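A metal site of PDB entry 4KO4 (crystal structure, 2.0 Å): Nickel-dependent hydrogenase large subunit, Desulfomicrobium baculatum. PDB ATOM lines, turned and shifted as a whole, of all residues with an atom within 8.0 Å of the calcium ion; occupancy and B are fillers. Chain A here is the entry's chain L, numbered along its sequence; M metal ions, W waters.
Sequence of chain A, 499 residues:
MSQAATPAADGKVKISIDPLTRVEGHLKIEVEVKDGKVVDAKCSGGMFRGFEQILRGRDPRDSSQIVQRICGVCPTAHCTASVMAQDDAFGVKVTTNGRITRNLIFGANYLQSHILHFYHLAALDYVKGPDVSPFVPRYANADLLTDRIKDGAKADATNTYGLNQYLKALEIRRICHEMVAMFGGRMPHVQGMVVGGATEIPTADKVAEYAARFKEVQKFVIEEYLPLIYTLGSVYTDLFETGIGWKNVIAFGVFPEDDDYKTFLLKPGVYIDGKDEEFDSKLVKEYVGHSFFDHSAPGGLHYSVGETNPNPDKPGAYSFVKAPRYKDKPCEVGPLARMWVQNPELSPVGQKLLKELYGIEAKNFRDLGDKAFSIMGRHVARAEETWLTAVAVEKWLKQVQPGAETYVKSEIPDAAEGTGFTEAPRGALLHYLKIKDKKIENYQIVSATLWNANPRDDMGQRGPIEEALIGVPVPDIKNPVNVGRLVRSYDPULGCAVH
Water W3 lies within hydrogen-bond range of the side-chain carboxylate (OE2) of Glu 286, the side-chain amide oxygen (OE1) of Gln 444 and the side-chain amino group (NZ) of Lys 322. Water W2 bridges the side-chain carboxylate (OE2) of Glu 52 (2.7 Å) and the side-chain amino group (NZ) of Lys 322 (3.2 Å).
Water W1 is bound to the calcium ion, 2.3 Å away. Water W3 binds the calcium ion (2.3 Å). OE1 of Glu 52 binds the calcium ion (2.3 Å). The calcium ion is bound by O of Ile 445 (2.3 Å). Water W2 is bound to the calcium ion, at 2.4 Å. The calcium ion is bound by NE2 of His 499. The calcium ion has six donor atoms within binding distance.
Within 4 Å of the calcium ion: Glu 52, Ile 445 and His 499.
The side-chain hydroxyl of Thr 308 lies within hydrogen-bond range of the side-chain carboxylate of Glu 52 (2.6 Å). O of Cys 496 is in hydrogen-bond range of ND1 of His 499, 2.7 Å away.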
ATOM      1  N   PHE A  48       6.868 -17.936  -9.408  1.00  0.00           N
ATOM      2  CA  PHE A  48       5.958 -18.854 -10.089  1.00  0.00           C
ATOM      3  C   PHE A  48       6.223 -18.876 -11.579  1.00  0.00           C
ATOM      4  O   PHE A  48       6.449 -17.817 -12.175  1.00  0.00           O
ATOM      5  CB  PHE A  48       4.497 -18.426  -9.827  1.00  0.00           C
ATOM      6  CG  PHE A  48       3.449 -19.207 -10.612  1.00  0.00           C
ATOM      7  CD1 PHE A  48       3.025 -20.463 -10.178  1.00  0.00           C
ATOM      8  CD2 PHE A  48       2.866 -18.666 -11.758  1.00  0.00           C
ATOM      9  CE1 PHE A  48       2.050 -21.179 -10.887  1.00  0.00           C
ATOM     10  CE2 PHE A  48       1.889 -19.381 -12.477  1.00  0.00           C
ATOM     11  CZ  PHE A  48       1.487 -20.645 -12.029  1.00  0.00           C
ATOM     12  N   GLU A  52       2.305 -26.452 -15.103  1.00  0.00           N
ATOM     13  CA  GLU A  52       1.055 -27.160 -15.316  1.00  0.00           C
ATOM     14  C   GLU A  52       0.196 -26.464 -16.378  1.00  0.00           C
ATOM     15  O   GLU A  52      -0.527 -27.131 -17.125  1.00  0.00           O
ATOM     16  CB  GLU A  52       0.315 -27.321 -13.986  1.00  0.00           C
ATOM     17  CG  GLU A  52       1.077 -28.232 -13.007  1.00  0.00           C
ATOM     18  CD  GLU A  52       0.777 -27.934 -11.551  1.00  0.00           C
ATOM     19  OE1 GLU A  52       0.885 -28.856 -10.709  1.00  0.00           O
ATOM     20  OE2 GLU A  52       0.443 -26.776 -11.242  1.00  0.00           O
ATOM     21  N   GLU A 286      -4.680 -31.107  -1.971  1.00  0.00           N
ATOM     22  CA  GLU A 286      -4.063 -29.800  -1.819  1.00  0.00           C
ATOM     23  C   GLU A 286      -5.067 -28.714  -1.477  1.00  0.00           C
ATOM     24  O   GLU A 286      -6.109 -28.591  -2.129  1.00  0.00           O
ATOM     25  CB  GLU A 286      -3.297 -29.401  -3.078  1.00  0.00           C
ATOM     26  CG  GLU A 286      -2.134 -30.321  -3.378  1.00  0.00           C
ATOM     27  CD  GLU A 286      -1.439 -29.929  -4.653  1.00  0.00           C
ATOM     28  OE1 GLU A 286      -0.307 -29.405  -4.556  1.00  0.00           O
ATOM     29  OE2 GLU A 286      -2.028 -30.127  -5.753  1.00  0.00           O
ATOM     30  N   PHE A 293      -3.610 -19.029  -5.384  1.00  0.00           N
ATOM     31  CA  PHE A 293      -4.350 -19.842  -6.356  1.00  0.00           C
ATOM     32  C   PHE A 293      -5.842 -19.858  -6.070  1.00  0.00           C
ATOM     33  O   PHE A 293      -6.250 -19.838  -4.911  1.00  0.00           O
ATOM     34  CB  PHE A 293      -3.849 -21.296  -6.393  1.00  0.00           C
ATOM     35  CG  PHE A 293      -2.440 -21.405  -6.887  1.00  0.00           C
ATOM     36  CD1 PHE A 293      -2.166 -21.354  -8.264  1.00  0.00           C
ATOM     37  CD2 PHE A 293      -1.391 -21.508  -5.985  1.00  0.00           C
ATOM     38  CE1 PHE A 293      -0.865 -21.390  -8.722  1.00  0.00           C
ATOM     39  CE2 PHE A 293      -0.072 -21.560  -6.439  1.00  0.00           C
ATOM     40  CZ  PHE A 293       0.196 -21.496  -7.813  1.00  0.00           C
ATOM     41  N   TYR A 303      -5.137 -34.454  -6.467  1.00  0.00           N
ATOM     42  CA  TYR A 303      -4.297 -34.036  -7.594  1.00  0.00           C
ATOM     43  C   TYR A 303      -4.873 -34.449  -8.967  1.00  0.00           C
ATOM     44  O   TYR A 303      -4.628 -33.766  -9.954  1.00  0.00           O
ATOM     45  CB  TYR A 303      -2.843 -34.538  -7.431  1.00  0.00           C
ATOM     46  CG  TYR A 303      -2.748 -36.029  -7.333  1.00  0.00           C
ATOM     47  CD1 TYR A 303      -2.809 -36.826  -8.484  1.00  0.00           C
ATOM     48  CD2 TYR A 303      -2.638 -36.657  -6.085  1.00  0.00           C
ATOM     49  CE1 TYR A 303      -2.739 -38.203  -8.404  1.00  0.00           C
ATOM     50  CE2 TYR A 303      -2.578 -38.043  -5.994  1.00  0.00           C
ATOM     51  CZ  TYR A 303      -2.634 -38.808  -7.162  1.00  0.00           C
ATOM     52  OH  TYR A 303      -2.573 -40.174  -7.048  1.00  0.00           O
ATOM     53  N   GLY A 306      -6.710 -31.605  -9.897  1.00  0.00           N
ATOM     54  CA  GLY A 306      -5.990 -30.394  -9.492  1.00  0.00           C
ATOM     55  C   GLY A 306      -6.221 -29.252 -10.482  1.00  0.00           C
ATOM     56  O   GLY A 306      -6.485 -29.474 -11.667  1.00  0.00           O
ATOM     57  N   GLU A 307      -6.107 -28.032  -9.973  1.00  0.00           N
ATOM     58  CA  GLU A 307      -6.338 -26.822 -10.756  1.00  0.00           C
ATOM     59  C   GLU A 307      -5.220 -25.844 -10.495  1.00  0.00           C
ATOM     60  O   GLU A 307      -4.780 -25.674  -9.356  1.00  0.00           O
ATOM     61  CB  GLU A 307      -7.669 -26.171 -10.375  1.00  0.00           C
ATOM     62  CG  GLU A 307      -8.905 -27.003 -10.682  1.00  0.00           C
ATOM     63  CD  GLU A 307     -10.173 -26.422 -10.067  1.00  0.00           C
ATOM     64  OE1 GLU A 307     -10.119 -25.303  -9.508  1.00  0.00           O
ATOM     65  OE2 GLU A 307     -11.225 -27.088 -10.151  1.00  0.00           O
ATOM     66  N   THR A 308      -4.759 -25.192 -11.565  1.00  0.00           N
ATOM     67  CA  THR A 308      -3.662 -24.238 -11.438  1.00  0.00           C
ATOM     68  C   THR A 308      -4.079 -22.917 -12.070  1.00  0.00           C
ATOM     69  O   THR A 308      -3.863 -22.671 -13.281  1.00  0.00           O
ATOM     70  CB  THR A 308      -2.368 -24.800 -12.014  1.00  0.00           C
ATOM     71  OG1 THR A 308      -2.084 -26.029 -11.339  1.00  0.00           O
ATOM     72  CG2 THR A 308      -1.198 -23.835 -11.787  1.00  0.00           C
ATOM     73  N   PHE A 320       3.319 -18.907  -3.253  1.00  0.00           N
ATOM     74  CA  PHE A 320       2.994 -19.643  -4.492  1.00  0.00           C
ATOM     75  C   PHE A 320       3.040 -21.158  -4.303  1.00  0.00           C
ATOM     76  O   PHE A 320       2.820 -21.908  -5.257  1.00  0.00           O
ATOM     77  CB  PHE A 320       3.894 -19.211  -5.650  1.00  0.00           C
ATOM     78  CG  PHE A 320       3.555 -17.855  -6.232  1.00  0.00           C
ATOM     79  CD1 PHE A 320       2.360 -17.638  -6.919  1.00  0.00           C
ATOM     80  CD2 PHE A 320       4.455 -16.807  -6.099  1.00  0.00           C
ATOM     81  CE1 PHE A 320       2.046 -16.379  -7.459  1.00  0.00           C
ATOM     82  CE2 PHE A 320       4.163 -15.535  -6.611  1.00  0.00           C
ATOM     83  CZ  PHE A 320       2.956 -15.325  -7.296  1.00  0.00           C
ATOM     84  N   LYS A 322       1.337 -24.458  -2.919  1.00  0.00           N
ATOM     85  CA  LYS A 322       0.063 -25.014  -2.420  1.00  0.00           C
ATOM     86  C   LYS A 322       0.328 -25.780  -1.123  1.00  0.00           C
ATOM     87  O   LYS A 322       1.483 -25.951  -0.721  1.00  0.00           O
ATOM     88  CB  LYS A 322      -0.599 -25.942  -3.457  1.00  0.00           C
ATOM     89  CG  LYS A 322      -0.961 -25.278  -4.800  1.00  0.00           C
ATOM     90  CD  LYS A 322      -1.723 -26.270  -5.690  1.00  0.00           C
ATOM     91  CE  LYS A 322      -2.174 -25.662  -7.021  1.00  0.00           C
ATOM     92  NZ  LYS A 322      -2.552 -26.736  -8.040  1.00  0.00           N
ATOM     93  N   LEU A 430       4.984 -37.092  -7.243  1.00  0.00           N
ATOM     94  CA  LEU A 430       4.168 -37.696  -8.291  1.00  0.00           C
ATOM     95  C   LEU A 430       3.848 -36.686  -9.384  1.00  0.00           C
ATOM     96  O   LEU A 430       3.795 -35.466  -9.139  1.00  0.00           O
ATOM     97  CB  LEU A 430       2.877 -38.336  -7.719  1.00  0.00           C
ATOM     98  CG  LEU A 430       1.822 -37.413  -7.100  1.00  0.00           C
ATOM     99  CD1 LEU A 430       0.852 -36.839  -8.156  1.00  0.00           C
ATOM    100  CD2 LEU A 430       1.047 -38.185  -6.019  1.00  0.00           C
ATOM    101  N   TYR A 443      -2.100 -31.667 -16.367  1.00  0.00           N
ATOM    102  CA  TYR A 443      -0.884 -32.259 -15.824  1.00  0.00           C
ATOM    103  C   TYR A 443      -0.710 -31.643 -14.446  1.00  0.00           C
ATOM    104  O   TYR A 443      -0.664 -30.425 -14.316  1.00  0.00           O
ATOM    105  CB  TYR A 443       0.297 -31.916 -16.716  1.00  0.00           C
ATOM    106  CG  TYR A 443       1.510 -32.813 -16.569  1.00  0.00           C
ATOM    107  CD1 TYR A 443       2.353 -32.719 -15.448  1.00  0.00           C
ATOM    108  CD2 TYR A 443       1.836 -33.746 -17.567  1.00  0.00           C
ATOM    109  CE1 TYR A 443       3.482 -33.544 -15.334  1.00  0.00           C
ATOM    110  CE2 TYR A 443       2.957 -34.557 -17.460  1.00  0.00           C
ATOM    111  CZ  TYR A 443       3.773 -34.455 -16.331  1.00  0.00           C
ATOM    112  OH  TYR A 443       4.884 -35.264 -16.221  1.00  0.00           O
ATOM    113  N   GLN A 444      -0.636 -32.484 -13.418  1.00  0.00           N
ATOM    114  CA  GLN A 444      -0.562 -31.983 -12.045  1.00  0.00           C
ATOM    115  C   GLN A 444       0.646 -32.595 -11.348  1.00  0.00           C
ATOM    116  O   GLN A 444       0.830 -33.813 -11.342  1.00  0.00           O
ATOM    117  CB  GLN A 444      -1.864 -32.256 -11.281  1.00  0.00           C
ATOM    118  CG  GLN A 444      -3.051 -31.384 -11.748  1.00  0.00           C
ATOM    119  CD  GLN A 444      -2.877 -29.921 -11.372  1.00  0.00           C
ATOM    120  OE1 GLN A 444      -2.542 -29.602 -10.229  1.00  0.00           O
ATOM    121  NE2 GLN A 444      -3.090 -29.030 -12.330  1.00  0.00           N
ATOM    122  N   ILE A 445       1.476 -31.725 -10.791  1.00  0.00           N
ATOM    123  CA  ILE A 445       2.707 -32.121 -10.128  1.00  0.00           C
ATOM    124  C   ILE A 445       2.578 -31.913  -8.620  1.00  0.00           C
ATOM    125  O   ILE A 445       2.204 -30.826  -8.178  1.00  0.00           O
ATOM    126  CB  ILE A 445       3.893 -31.300 -10.692  1.00  0.00           C
ATOM    127  CG1 ILE A 445       4.120 -31.679 -12.165  1.00  0.00           C
ATOM    128  CG2 ILE A 445       5.146 -31.537  -9.845  1.00  0.00           C
ATOM    129  CD1 ILE A 445       4.588 -30.559 -13.053  1.00  0.00           C
ATOM    130  N   VAL A 446       2.860 -32.960  -7.834  1.00  0.00           N
ATOM    131  CA  VAL A 446       2.867 -32.865  -6.373  1.00  0.00           C
ATOM    132  C   VAL A 446       4.290 -33.246  -6.020  1.00  0.00           C
ATOM    133  O   VAL A 446       4.664 -34.403  -6.099  1.00  0.00           O
ATOM    134  CB  VAL A 446       1.785 -33.800  -5.735  1.00  0.00           C
ATOM    135  CG1 VAL A 446       1.826 -33.721  -4.211  1.00  0.00           C
ATOM    136  CG2 VAL A 446       0.394 -33.436  -6.274  1.00  0.00           C
ATOM    137  N   SER A 447       5.077 -32.231  -5.669  1.00  0.00           N
ATOM    138  CA  SER A 447       6.505 -32.410  -5.484  1.00  0.00           C
ATOM    139  C   SER A 447       6.927 -32.469  -4.033  1.00  0.00           C
ATOM    140  O   SER A 447       6.137 -32.255  -3.113  1.00  0.00           O
ATOM    141  CB  SER A 447       7.263 -31.263  -6.163  1.00  0.00           C
ATOM    142  OG  SER A 447       6.940 -30.028  -5.535  1.00  0.00           O
ATOM    143  N   LEU A 450       7.254 -29.122  -1.971  1.00  0.00           N
ATOM    144  CA  LEU A 450       5.840 -28.817  -1.800  1.00  0.00           C
ATOM    145  C   LEU A 450       5.301 -29.309  -0.430  1.00  0.00           C
ATOM    146  O   LEU A 450       4.582 -28.584   0.262  1.00  0.00           O
ATOM    147  CB  LEU A 450       5.011 -29.420  -2.938  1.00  0.00           C
ATOM    148  CG  LEU A 450       3.482 -29.415  -2.776  1.00  0.00           C
ATOM    149  CD1 LEU A 450       2.907 -28.002  -2.852  1.00  0.00           C
ATOM    150  CD2 LEU A 450       2.894 -30.268  -3.860  1.00  0.00           C
ATOM    151  N   CYS A 496      10.971 -26.595  -7.434  1.00  0.00           N
ATOM    152  CA  CYS A 496      10.093 -27.774  -7.334  1.00  0.00           C
ATOM    153  C   CYS A 496       8.812 -27.482  -6.604  1.00  0.00           C
ATOM    154  O   CYS A 496       7.752 -27.985  -6.983  1.00  0.00           O
ATOM    155  CB  CYS A 496      10.808 -28.923  -6.628  1.00  0.00           C
ATOM    156  SG  CYS A 496      12.148 -29.629  -7.557  1.00  0.00           S
ATOM    157  N   ALA A 497       8.911 -26.725  -5.509  1.00  0.00           N
ATOM    158  CA  ALA A 497       7.738 -26.520  -4.640  1.00  0.00           C
ATOM    159  C   ALA A 497       6.614 -25.837  -5.386  1.00  0.00           C
ATOM    160  O   ALA A 497       5.430 -26.137  -5.160  1.00  0.00           O
ATOM    161  CB  ALA A 497       8.113 -25.707  -3.380  1.00  0.00           C
ATOM    162  N   VAL A 498       6.972 -24.923  -6.292  1.00  0.00           N
ATOM    163  CA  VAL A 498       5.983 -24.048  -6.947  1.00  0.00           C
ATOM    164  C   VAL A 498       5.702 -24.456  -8.394  1.00  0.00           C
ATOM    165  O   VAL A 498       4.544 -24.492  -8.817  1.00  0.00           O
ATOM    166  CB  VAL A 498       6.419 -22.566  -6.946  1.00  0.00           C
ATOM    167  CG1 VAL A 498       5.396 -21.702  -7.720  1.00  0.00           C
ATOM    168  CG2 VAL A 498       6.600 -22.040  -5.521  1.00  0.00           C
ATOM    169  N   HIS A 499       6.771 -24.774  -9.123  1.00  0.00           N
ATOM    170  CA  HIS A 499       6.716 -25.119 -10.559  1.00  0.00           C
ATOM    171  C   HIS A 499       5.822 -24.149 -11.335  1.00  0.00           C
ATOM    172  O   HIS A 499       4.961 -24.570 -12.108  1.00  0.00           O
ATOM    173  CB  HIS A 499       6.370 -26.620 -10.810  1.00  0.00           C
ATOM    174  CG  HIS A 499       5.316 -27.194  -9.908  1.00  0.00           C
ATOM    175  ND1 HIS A 499       5.578 -27.581  -8.605  1.00  0.00           N
ATOM    176  CD2 HIS A 499       3.990 -27.416 -10.103  1.00  0.00           C
ATOM    177  CE1 HIS A 499       4.457 -28.012  -8.039  1.00  0.00           C
ATOM    178  NE2 HIS A 499       3.482 -27.924  -8.928  1.00  0.00           N
ATOM    179  OXT HIS A 499       5.956 -22.908 -11.180  1.00  0.00           O
HETATM  180 CA    CA M   1       1.224 -28.711  -8.423  1.00  0.00          CA
HETATM  181  O   HOH W   1       1.424 -28.265  -6.186  1.00  0.00           O
HETATM  182  O   HOH W   2       0.558 -26.428  -8.608  1.00  0.00           O
HETATM  183  O   HOH W   3      -0.942 -29.386  -7.983  1.00  0.00           O
